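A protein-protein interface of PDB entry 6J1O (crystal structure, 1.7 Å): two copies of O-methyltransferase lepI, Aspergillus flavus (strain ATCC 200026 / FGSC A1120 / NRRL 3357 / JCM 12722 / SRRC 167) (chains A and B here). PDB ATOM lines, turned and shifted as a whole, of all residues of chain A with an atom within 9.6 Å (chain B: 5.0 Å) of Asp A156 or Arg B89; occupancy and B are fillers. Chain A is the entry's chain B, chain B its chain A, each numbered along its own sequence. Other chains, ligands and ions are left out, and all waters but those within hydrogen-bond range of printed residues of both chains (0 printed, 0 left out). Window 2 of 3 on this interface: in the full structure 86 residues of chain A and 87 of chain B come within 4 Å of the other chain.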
ATOM      1  N   LEU A 145      11.534   2.420  22.600  1.00  0.00           N
ATOM      2  CA  LEU A 145      12.169   1.808  21.432  1.00  0.00           C
ATOM      3  C   LEU A 145      11.210   1.527  20.274  1.00  0.00           C
ATOM      4  O   LEU A 145      11.556   1.861  19.127  1.00  0.00           O
ATOM      5  CB  LEU A 145      12.908   0.535  21.862  1.00  0.00           C
ATOM      6  CG  LEU A 145      13.617  -0.236  20.744  1.00  0.00           C
ATOM      7  CD1 LEU A 145      14.826   0.540  20.213  1.00  0.00           C
ATOM      8  CD2 LEU A 145      14.040  -1.623  21.238  1.00  0.00           C
ATOM      9  N   PHE A 148      10.305   4.773  18.453  1.00  0.00           N
ATOM     10  CA  PHE A 148      11.534   5.307  17.872  1.00  0.00           C
ATOM     11  C   PHE A 148      11.864   4.601  16.566  1.00  0.00           C
ATOM     12  O   PHE A 148      12.112   5.251  15.542  1.00  0.00           O
ATOM     13  CB  PHE A 148      12.700   5.183  18.858  1.00  0.00           C
ATOM     14  CG  PHE A 148      14.037   5.523  18.254  1.00  0.00           C
ATOM     15  CD1 PHE A 148      14.402   6.847  18.041  1.00  0.00           C
ATOM     16  CD2 PHE A 148      14.923   4.526  17.890  1.00  0.00           C
ATOM     17  CE1 PHE A 148      15.628   7.161  17.477  1.00  0.00           C
ATOM     18  CE2 PHE A 148      16.146   4.835  17.323  1.00  0.00           C
ATOM     19  CZ  PHE A 148      16.500   6.156  17.121  1.00  0.00           C
ATOM     20  N   LEU A 149      11.856   3.263  16.578  1.00  0.00           N
ATOM     21  CA  LEU A 149      12.175   2.508  15.370  1.00  0.00           C
ATOM     22  C   LEU A 149      11.138   2.739  14.279  1.00  0.00           C
ATOM     23  O   LEU A 149      11.491   2.872  13.100  1.00  0.00           O
ATOM     24  CB  LEU A 149      12.286   1.017  15.687  1.00  0.00           C
ATOM     25  CG  LEU A 149      13.455   0.601  16.584  1.00  0.00           C
ATOM     26  CD1 LEU A 149      13.388  -0.900  16.870  1.00  0.00           C
ATOM     27  CD2 LEU A 149      14.793   0.973  15.959  1.00  0.00           C
ATOM     28  N   ARG A 152      11.476   6.116  12.514  1.00  0.00           N
ATOM     29  CA  ARG A 152      12.711   6.195  11.752  1.00  0.00           C
ATOM     30  C   ARG A 152      12.827   5.102  10.694  1.00  0.00           C
ATOM     31  O   ARG A 152      13.899   4.940  10.102  1.00  0.00           O
ATOM     32  CB  ARG A 152      13.896   6.137  12.711  1.00  0.00           C
ATOM     33  CG  ARG A 152      14.003   7.367  13.598  1.00  0.00           C
ATOM     34  CD  ARG A 152      14.606   8.526  12.822  1.00  0.00           C
ATOM     35  NE  ARG A 152      15.959   8.181  12.409  1.00  0.00           N
ATOM     36  CZ  ARG A 152      17.035   8.374  13.164  1.00  0.00           C
ATOM     37  NH1 ARG A 152      16.914   8.932  14.362  1.00  0.00           N
ATOM     38  NH2 ARG A 152      18.228   8.011  12.718  1.00  0.00           N
ATOM     39  N   LYS A 153      11.748   4.354  10.448  1.00  0.00           N
ATOM     40  CA  LYS A 153      11.721   3.304   9.427  1.00  0.00           C
ATOM     41  C   LYS A 153      12.812   2.263   9.668  1.00  0.00           C
ATOM     42  O   LYS A 153      13.484   1.810   8.738  1.00  0.00           O
ATOM     43  CB  LYS A 153      11.823   3.898   8.019  1.00  0.00           C
ATOM     44  CG  LYS A 153      10.716   4.892   7.698  1.00  0.00           C
ATOM     45  CD  LYS A 153      11.057   5.737   6.479  1.00  0.00           C
ATOM     46  CE  LYS A 153      11.328   4.875   5.255  1.00  0.00           C
ATOM     47  NZ  LYS A 153      11.694   5.703   4.071  1.00  0.00           N
ATOM     48  N   TYR A 154      12.998   1.899  10.942  1.00  0.00           N
ATOM     49  CA  TYR A 154      13.767   0.735  11.382  1.00  0.00           C
ATOM     50  C   TYR A 154      15.227   0.806  10.956  1.00  0.00           C
ATOM     51  O   TYR A 154      15.722  -0.061  10.224  1.00  0.00           O
ATOM     52  CB  TYR A 154      13.076  -0.542  10.885  1.00  0.00           C
ATOM     53  CG  TYR A 154      11.687  -0.603  11.469  1.00  0.00           C
ATOM     54  CD1 TYR A 154      11.479  -1.111  12.745  1.00  0.00           C
ATOM     55  CD2 TYR A 154      10.597  -0.071  10.786  1.00  0.00           C
ATOM     56  CE1 TYR A 154      10.224  -1.118  13.309  1.00  0.00           C
ATOM     57  CE2 TYR A 154       9.332  -0.077  11.340  1.00  0.00           C
ATOM     58  CZ  TYR A 154       9.151  -0.609  12.604  1.00  0.00           C
ATOM     59  OH  TYR A 154       7.900  -0.610  13.172  1.00  0.00           O
ATOM     60  N   PRO A 155      15.958   1.808  11.436  1.00  0.00           N
ATOM     61  CA  PRO A 155      17.374   1.925  11.096  1.00  0.00           C
ATOM     62  C   PRO A 155      18.232   0.969  11.912  1.00  0.00           C
ATOM     63  O   PRO A 155      17.863   0.521  13.001  1.00  0.00           O
ATOM     64  CB  PRO A 155      17.690   3.378  11.461  1.00  0.00           C
ATOM     65  CG  PRO A 155      16.816   3.630  12.662  1.00  0.00           C
ATOM     66  CD  PRO A 155      15.535   2.843  12.400  1.00  0.00           C
ATOM     67  N   ASP A 156      19.406   0.677  11.371  1.00  0.00           N
ATOM     68  CA  ASP A 156      20.443   0.039  12.168  1.00  0.00           C
ATOM     69  C   ASP A 156      21.007   1.064  13.142  1.00  0.00           C
ATOM     70  O   ASP A 156      21.514   2.110  12.724  1.00  0.00           O
ATOM     71  CB  ASP A 156      21.553  -0.517  11.279  1.00  0.00           C
ATOM     72  CG  ASP A 156      21.111  -1.708  10.454  1.00  0.00           C
ATOM     73  OD1 ASP A 156      20.101  -2.352  10.810  1.00  0.00           O
ATOM     74  OD2 ASP A 156      21.786  -2.010   9.448  1.00  0.00           O
ATOM     75  N   ILE A 157      20.899   0.788  14.439  1.00  0.00           N
ATOM     76  CA  ILE A 157      21.366   1.732  15.448  1.00  0.00           C
ATOM     77  C   ILE A 157      22.873   1.582  15.601  1.00  0.00           C
ATOM     78  O   ILE A 157      23.381   0.475  15.823  1.00  0.00           O
ATOM     79  CB  ILE A 157      20.639   1.507  16.783  1.00  0.00           C
ATOM     80  CG1 ILE A 157      19.145   1.816  16.631  1.00  0.00           C
ATOM     81  CG2 ILE A 157      21.259   2.361  17.878  1.00  0.00           C
ATOM     82  CD1 ILE A 157      18.317   1.438  17.844  1.00  0.00           C
ATOM     83  N   VAL A 158      23.594   2.697  15.475  1.00  0.00           N
ATOM     84  CA  VAL A 158      25.050   2.657  15.381  1.00  0.00           C
ATOM     85  C   VAL A 158      25.711   3.771  16.185  1.00  0.00           C
ATOM     86  O   VAL A 158      26.942   3.826  16.272  1.00  0.00           O
ATOM     87  CB  VAL A 158      25.497   2.746  13.909  1.00  0.00           C
ATOM     88  CG1 VAL A 158      25.024   1.530  13.121  1.00  0.00           C
ATOM     89  CG2 VAL A 158      24.970   4.032  13.283  1.00  0.00           C
ATOM     90  N   ASP A 159      24.915   4.672  16.759  1.00  0.00           N
ATOM     91  CA  ASP A 159      25.417   5.921  17.330  1.00  0.00           C
ATOM     92  C   ASP A 159      24.838   6.119  18.725  1.00  0.00           C
ATOM     93  O   ASP A 159      23.618   6.098  18.899  1.00  0.00           O
ATOM     94  CB  ASP A 159      25.053   7.098  16.410  1.00  0.00           C
ATOM     95  CG  ASP A 159      25.560   8.446  16.912  1.00  0.00           C
ATOM     96  OD1 ASP A 159      26.231   8.520  17.965  1.00  0.00           O
ATOM     97  OD2 ASP A 159      25.280   9.451  16.227  1.00  0.00           O
ATOM     98  N   ALA A 160      25.714   6.328  19.716  1.00  0.00           N
ATOM     99  CA  ALA A 160      25.257   6.536  21.085  1.00  0.00           C
ATOM    100  C   ALA A 160      24.419   7.799  21.239  1.00  0.00           C
ATOM    101  O   ALA A 160      23.653   7.909  22.202  1.00  0.00           O
ATOM    102  CB  ALA A 160      26.457   6.597  22.033  1.00  0.00           C
ATOM    103  N   ASP A 162      22.159   8.767  18.932  1.00  0.00           N
ATOM    104  CA  ASP A 162      20.983   8.655  18.078  1.00  0.00           C
ATOM    105  C   ASP A 162      20.333   7.279  18.277  1.00  0.00           C
ATOM    106  O   ASP A 162      20.357   6.415  17.404  1.00  0.00           O
ATOM    107  CB  ASP A 162      21.344   8.882  16.609  1.00  0.00           C
ATOM    108  CG  ASP A 162      20.127   8.878  15.707  1.00  0.00           C
ATOM    109  OD1 ASP A 162      19.009   9.078  16.229  1.00  0.00           O
ATOM    110  OD2 ASP A 162      20.286   8.649  14.486  1.00  0.00           O
ATOM    111  N   THR A 163      19.734   7.075  19.447  1.00  0.00           N
ATOM    112  CA  THR A 163      19.054   5.818  19.736  1.00  0.00           C
ATOM    113  C   THR A 163      17.822   6.124  20.587  1.00  0.00           C
ATOM    114  O   THR A 163      17.407   7.280  20.720  1.00  0.00           O
ATOM    115  CB  THR A 163      20.035   4.827  20.379  1.00  0.00           C
ATOM    116  OG1 THR A 163      19.401   3.554  20.543  1.00  0.00           O
ATOM    117  CG2 THR A 163      20.554   5.349  21.726  1.00  0.00           C
ATOM    118  N   MET A 343      21.833  -1.717  22.925  1.00  0.00           N
ATOM    119  CA  MET A 343      21.477  -1.045  21.681  1.00  0.00           C
ATOM    120  C   MET A 343      20.595   0.163  21.959  1.00  0.00           C
ATOM    121  O   MET A 343      20.877   1.280  21.499  1.00  0.00           O
ATOM    122  CB  MET A 343      20.763  -2.014  20.735  1.00  0.00           C
ATOM    123  CG  MET A 343      20.392  -1.386  19.403  1.00  0.00           C
ATOM    124  SD  MET A 343      19.414  -2.519  18.395  1.00  0.00           S
ATOM    125  CE  MET A 343      17.830  -2.411  19.228  1.00  0.00           C
ATOM    126  N   GLY A 347      23.602   2.635  22.148  1.00  0.00           N
ATOM    127  CA  GLY A 347      24.051   2.465  20.781  1.00  0.00           C
ATOM    128  C   GLY A 347      25.095   1.392  20.562  1.00  0.00           C
ATOM    129  O   GLY A 347      25.644   1.305  19.459  1.00  0.00           O
ATOM    130  N   SER A 348      25.372   0.548  21.556  1.00  0.00           N
ATOM    131  CA  SER A 348      26.426  -0.450  21.463  1.00  0.00           C
ATOM    132  C   SER A 348      25.814  -1.825  21.169  1.00  0.00           C
ATOM    133  O   SER A 348      24.684  -1.917  20.676  1.00  0.00           O
ATOM    134  CB  SER A 348      27.265  -0.416  22.750  1.00  0.00           C
ATOM    135  OG  SER A 348      26.483  -0.726  23.894  1.00  0.00           O
ATOM    136  N   LYS A 349      26.550  -2.897  21.463  1.00  0.00           N
ATOM    137  CA  LYS A 349      26.149  -4.228  21.021  1.00  0.00           C
ATOM    138  C   LYS A 349      26.977  -5.278  21.752  1.00  0.00           C
ATOM    139  O   LYS A 349      28.111  -5.014  22.158  1.00  0.00           O
ATOM    140  CB  LYS A 349      26.338  -4.379  19.504  1.00  0.00           C
ATOM    141  CG  LYS A 349      27.810  -4.365  19.067  1.00  0.00           C
ATOM    142  CD  LYS A 349      27.961  -4.277  17.545  1.00  0.00           C
ATOM    143  CE  LYS A 349      27.455  -5.524  16.839  1.00  0.00           C
ATOM    144  NZ  LYS A 349      27.979  -6.795  17.414  1.00  0.00           N
ATOM    145  N   GLU B  79      18.264 -11.893   6.602  1.00  0.00           N
ATOM    146  CA  GLU B  79      18.291 -10.973   5.470  1.00  0.00           C
ATOM    147  C   GLU B  79      16.990 -11.031   4.677  1.00  0.00           C
ATOM    148  O   GLU B  79      16.450  -9.990   4.277  1.00  0.00           O
ATOM    149  CB  GLU B  79      19.491 -11.290   4.575  1.00  0.00           C
ATOM    150  CG  GLU B  79      20.855 -11.023   5.220  1.00  0.00           C
ATOM    151  CD  GLU B  79      21.204 -11.997   6.346  1.00  0.00           C
ATOM    152  OE1 GLU B  79      20.634 -13.115   6.388  1.00  0.00           O
ATOM    153  OE2 GLU B  79      22.048 -11.641   7.197  1.00  0.00           O
ATOM    154  N   ALA B  82      14.310  -9.280   6.785  1.00  0.00           N
ATOM    155  CA  ALA B  82      14.545  -7.840   6.813  1.00  0.00           C
ATOM    156  C   ALA B  82      14.111  -7.198   5.504  1.00  0.00           C
ATOM    157  O   ALA B  82      13.382  -6.200   5.497  1.00  0.00           O
ATOM    158  CB  ALA B  82      16.022  -7.555   7.087  1.00  0.00           C
ATOM    159  N   ASP B  83      14.542  -7.773   4.380  1.00  0.00           N
ATOM    160  CA  ASP B  83      14.191  -7.203   3.084  1.00  0.00           C
ATOM    161  C   ASP B  83      12.689  -7.257   2.845  1.00  0.00           C
ATOM    162  O   ASP B  83      12.097  -6.284   2.363  1.00  0.00           O
ATOM    163  CB  ASP B  83      14.946  -7.931   1.974  1.00  0.00           C
ATOM    164  CG  ASP B  83      16.444  -7.695   2.033  1.00  0.00           C
ATOM    165  OD1 ASP B  83      16.889  -6.859   2.852  1.00  0.00           O
ATOM    166  OD2 ASP B  83      17.178  -8.358   1.269  1.00  0.00           O
ATOM    167  N   CYS B  87      12.957  -3.713   7.169  1.00  0.00           N
ATOM    168  CA  CYS B  87      13.701  -3.508   8.403  1.00  0.00           C
ATOM    169  C   CYS B  87      15.189  -3.509   8.094  1.00  0.00           C
ATOM    170  O   CYS B  87      15.646  -4.239   7.211  1.00  0.00           O
ATOM    171  CB  CYS B  87      13.366  -4.605   9.429  1.00  0.00           C
ATOM    172  SG  CYS B  87      14.131  -4.375  11.063  1.00  0.00           S
ATOM    173  N   GLY B  88      15.947  -2.680   8.813  1.00  0.00           N
ATOM    174  CA  GLY B  88      17.391  -2.744   8.720  1.00  0.00           C
ATOM    175  C   GLY B  88      17.897  -4.150   8.965  1.00  0.00           C
ATOM    176  O   GLY B  88      17.376  -4.858   9.833  1.00  0.00           O
ATOM    177  N   ARG B  89      18.901  -4.575   8.195  1.00  0.00           N
ATOM    178  CA  ARG B  89      19.339  -5.967   8.255  1.00  0.00           C
ATOM    179  C   ARG B  89      19.981  -6.308   9.595  1.00  0.00           C
ATOM    180  O   ARG B  89      19.739  -7.386  10.150  1.00  0.00           O
ATOM    181  CB  ARG B  89      20.309  -6.261   7.114  1.00  0.00           C
ATOM    182  CG  ARG B  89      19.637  -6.420   5.761  1.00  0.00           C
ATOM    183  CD  ARG B  89      20.617  -6.969   4.740  1.00  0.00           C
ATOM    184  NE  ARG B  89      19.956  -7.367   3.500  1.00  0.00           N
ATOM    185  CZ  ARG B  89      20.582  -7.931   2.474  1.00  0.00           C
ATOM    186  NH1 ARG B  89      21.887  -8.164   2.540  1.00  0.00           N
ATOM    187  NH2 ARG B  89      19.904  -8.267   1.385  1.00  0.00           N
ATOM    188  N   GLU B  90      20.812  -5.412  10.128  1.00  0.00           N
ATOM    189  CA  GLU B  90      21.449  -5.698  11.408  1.00  0.00           C
ATOM    190  C   GLU B  90      20.432  -5.657  12.539  1.00  0.00           C
ATOM    191  O   GLU B  90      20.430  -6.533  13.416  1.00  0.00           O
ATOM    192  CB  GLU B  90      22.591  -4.713  11.660  1.00  0.00           C
ATOM    193  CG  GLU B  90      23.316  -4.910  12.991  1.00  0.00           C
ATOM    194  CD  GLU B  90      24.169  -6.171  13.046  1.00  0.00           C
ATOM    195  OE1 GLU B  90      24.977  -6.291  13.993  1.00  0.00           O
ATOM    196  OE2 GLU B  90      24.053  -7.034  12.148  1.00  0.00           O
ATOM    197  N   LEU B  91      19.541  -4.663  12.511  1.00  0.00           N
ATOM    198  CA  LEU B  91      18.449  -4.598  13.476  1.00  0.00           C
ATOM    199  C   LEU B  91      17.614  -5.872  13.442  1.00  0.00           C
ATOM    200  O   LEU B  91      17.300  -6.450  14.490  1.00  0.00           O
ATOM    201  CB  LEU B  91      17.578  -3.375  13.197  1.00  0.00           C
ATOM    202  CG  LEU B  91      16.304  -3.223  14.032  1.00  0.00           C
ATOM    203  CD1 LEU B  91      16.637  -3.174  15.518  1.00  0.00           C
ATOM    204  CD2 LEU B  91      15.558  -1.974  13.614  1.00  0.00           C
ATOM    205  N   MET B  92      17.253  -6.331  12.239  1.00  0.00           N
ATOM    206  CA  MET B  92      16.449  -7.543  12.129  1.00  0.00           C
ATOM    207  C   MET B  92      17.195  -8.750  12.680  1.00  0.00           C
ATOM    208  O   MET B  92      16.618  -9.562  13.410  1.00  0.00           O
ATOM    209  CB  MET B  92      16.047  -7.779  10.671  1.00  0.00           C
ATOM    210  CG  MET B  92      15.305  -9.086  10.447  1.00  0.00           C
ATOM    211  SD  MET B  92      13.682  -9.140  11.229  1.00  0.00           S
ATOM    212  CE  MET B  92      12.755  -8.061  10.170  1.00  0.00           C
ATOM    213  N   SER B  93      18.484  -8.879  12.356  1.00  0.00           N
ATOM    214  CA  SER B  93      19.260 -10.011  12.855  1.00  0.00           C
ATOM    215  C   SER B  93      19.294 -10.031  14.381  1.00  0.00           C
ATOM    216  O   SER B  93      19.089 -11.080  15.003  1.00  0.00           O
ATOM    217  CB  SER B  93      20.681  -9.966  12.296  1.00  0.00           C
ATOM    218  OG  SER B  93      21.443 -11.062  12.782  1.00  0.00           O
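The backbone NH (N) of Gly B88 sits at hydrogen-bond distance from the backbone carbonyl oxygen (O) of Tyr A154 (3.0 Å). The backbone NH (N) of Glu B90 sits at hydrogen-bond distance from the side-chain carboxylate (OD1) of Asp A156, at 3.2 Å. N of Leu B91 is in hydrogen-bond range of OD1 of Asp A156 (2.9 Å).
The backbone carbonyl oxygen (O) of Ala B82 lies within hydrogen-bond range of the backbone NH (N) of Cys B87 (3.0 Å). The guanidinium group (NH2) of Arg B89 lies within salt-bridge range of the side-chain carboxylate (OD2) of Asp B83, at 2.7 Å. N of Tyr A154 sits at hydrogen-bond distance from O of Leu A149 (2.8 Å). O of Met A343 is in hydrogen-bond range of OG1 of Thr A163, 2.9 Å away.
Among the printed residues, pairs that only touch across the chains: Asp A156 with Gly B88 (3.4 Å), Pro A155 with Leu B91 (3.5 Å), Asp A156 with Arg B89 (3.6 Å), Leu A149 with Leu B91 (3.8 Å), Lys A349 with Glu B90 (3.9 Å), Tyr A154 with Leu B91 (3.9 Å), Tyr A154 with Cys B87 (3.9 Å) and Met A343 with Leu B91 (3.97 Å).
Of the printed residues of chain B, Tyr A154 touches Cys B87, Gly B88 and Leu B91. Of the printed residues of chain B, Pro A155 touches Leu B91 (3.5 Å). Of chain B, only Gly B88, Arg B89, Glu B90 and Leu B91 come within 4 Å of Asp A156. Ile A157 touches none of the printed residues of chain B. Printed residues of chain B within 4 Å of Lys A349: Glu B90. Of the printed residues of chain A, Cys B87 touches Tyr A154. Gly B88 touches just these residues of chain A: Tyr A154 and Asp A156. Of chain A, only Asp A156 comes within 4 Å of Arg B89. Of the printed residues of chain A, Glu B90 touches Asp A156 and Lys A349. Ser B93 touches none of the printed residues of chain A. The nearest residue of chain A that does not touch Arg B89 is Tyr A154 (5.9 Å). The nearest printed residue of chain A that does not touch Leu B91 is Ile A157 (5.4 Å).
Of the 18 printed residues of chain A, 6 touch a printed residue of chain B. Hydrophobic or aromatic side chains of chain A within 4 Å of the printed part of chain B: Leu A149, Tyr A154 and Met A343. Along chain A the printed residues that touch a printed residue of chain B span positions 149 to 349. Of the 10 printed residues of chain B, 5 touch a printed residue of chain A. Among the printed residues, 11 pairs touch across the chains.
No position is printed for both chains. Of the 11 pairs that touch across the chains among the printed residues, none has its exchanged pair printed and touching as well.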
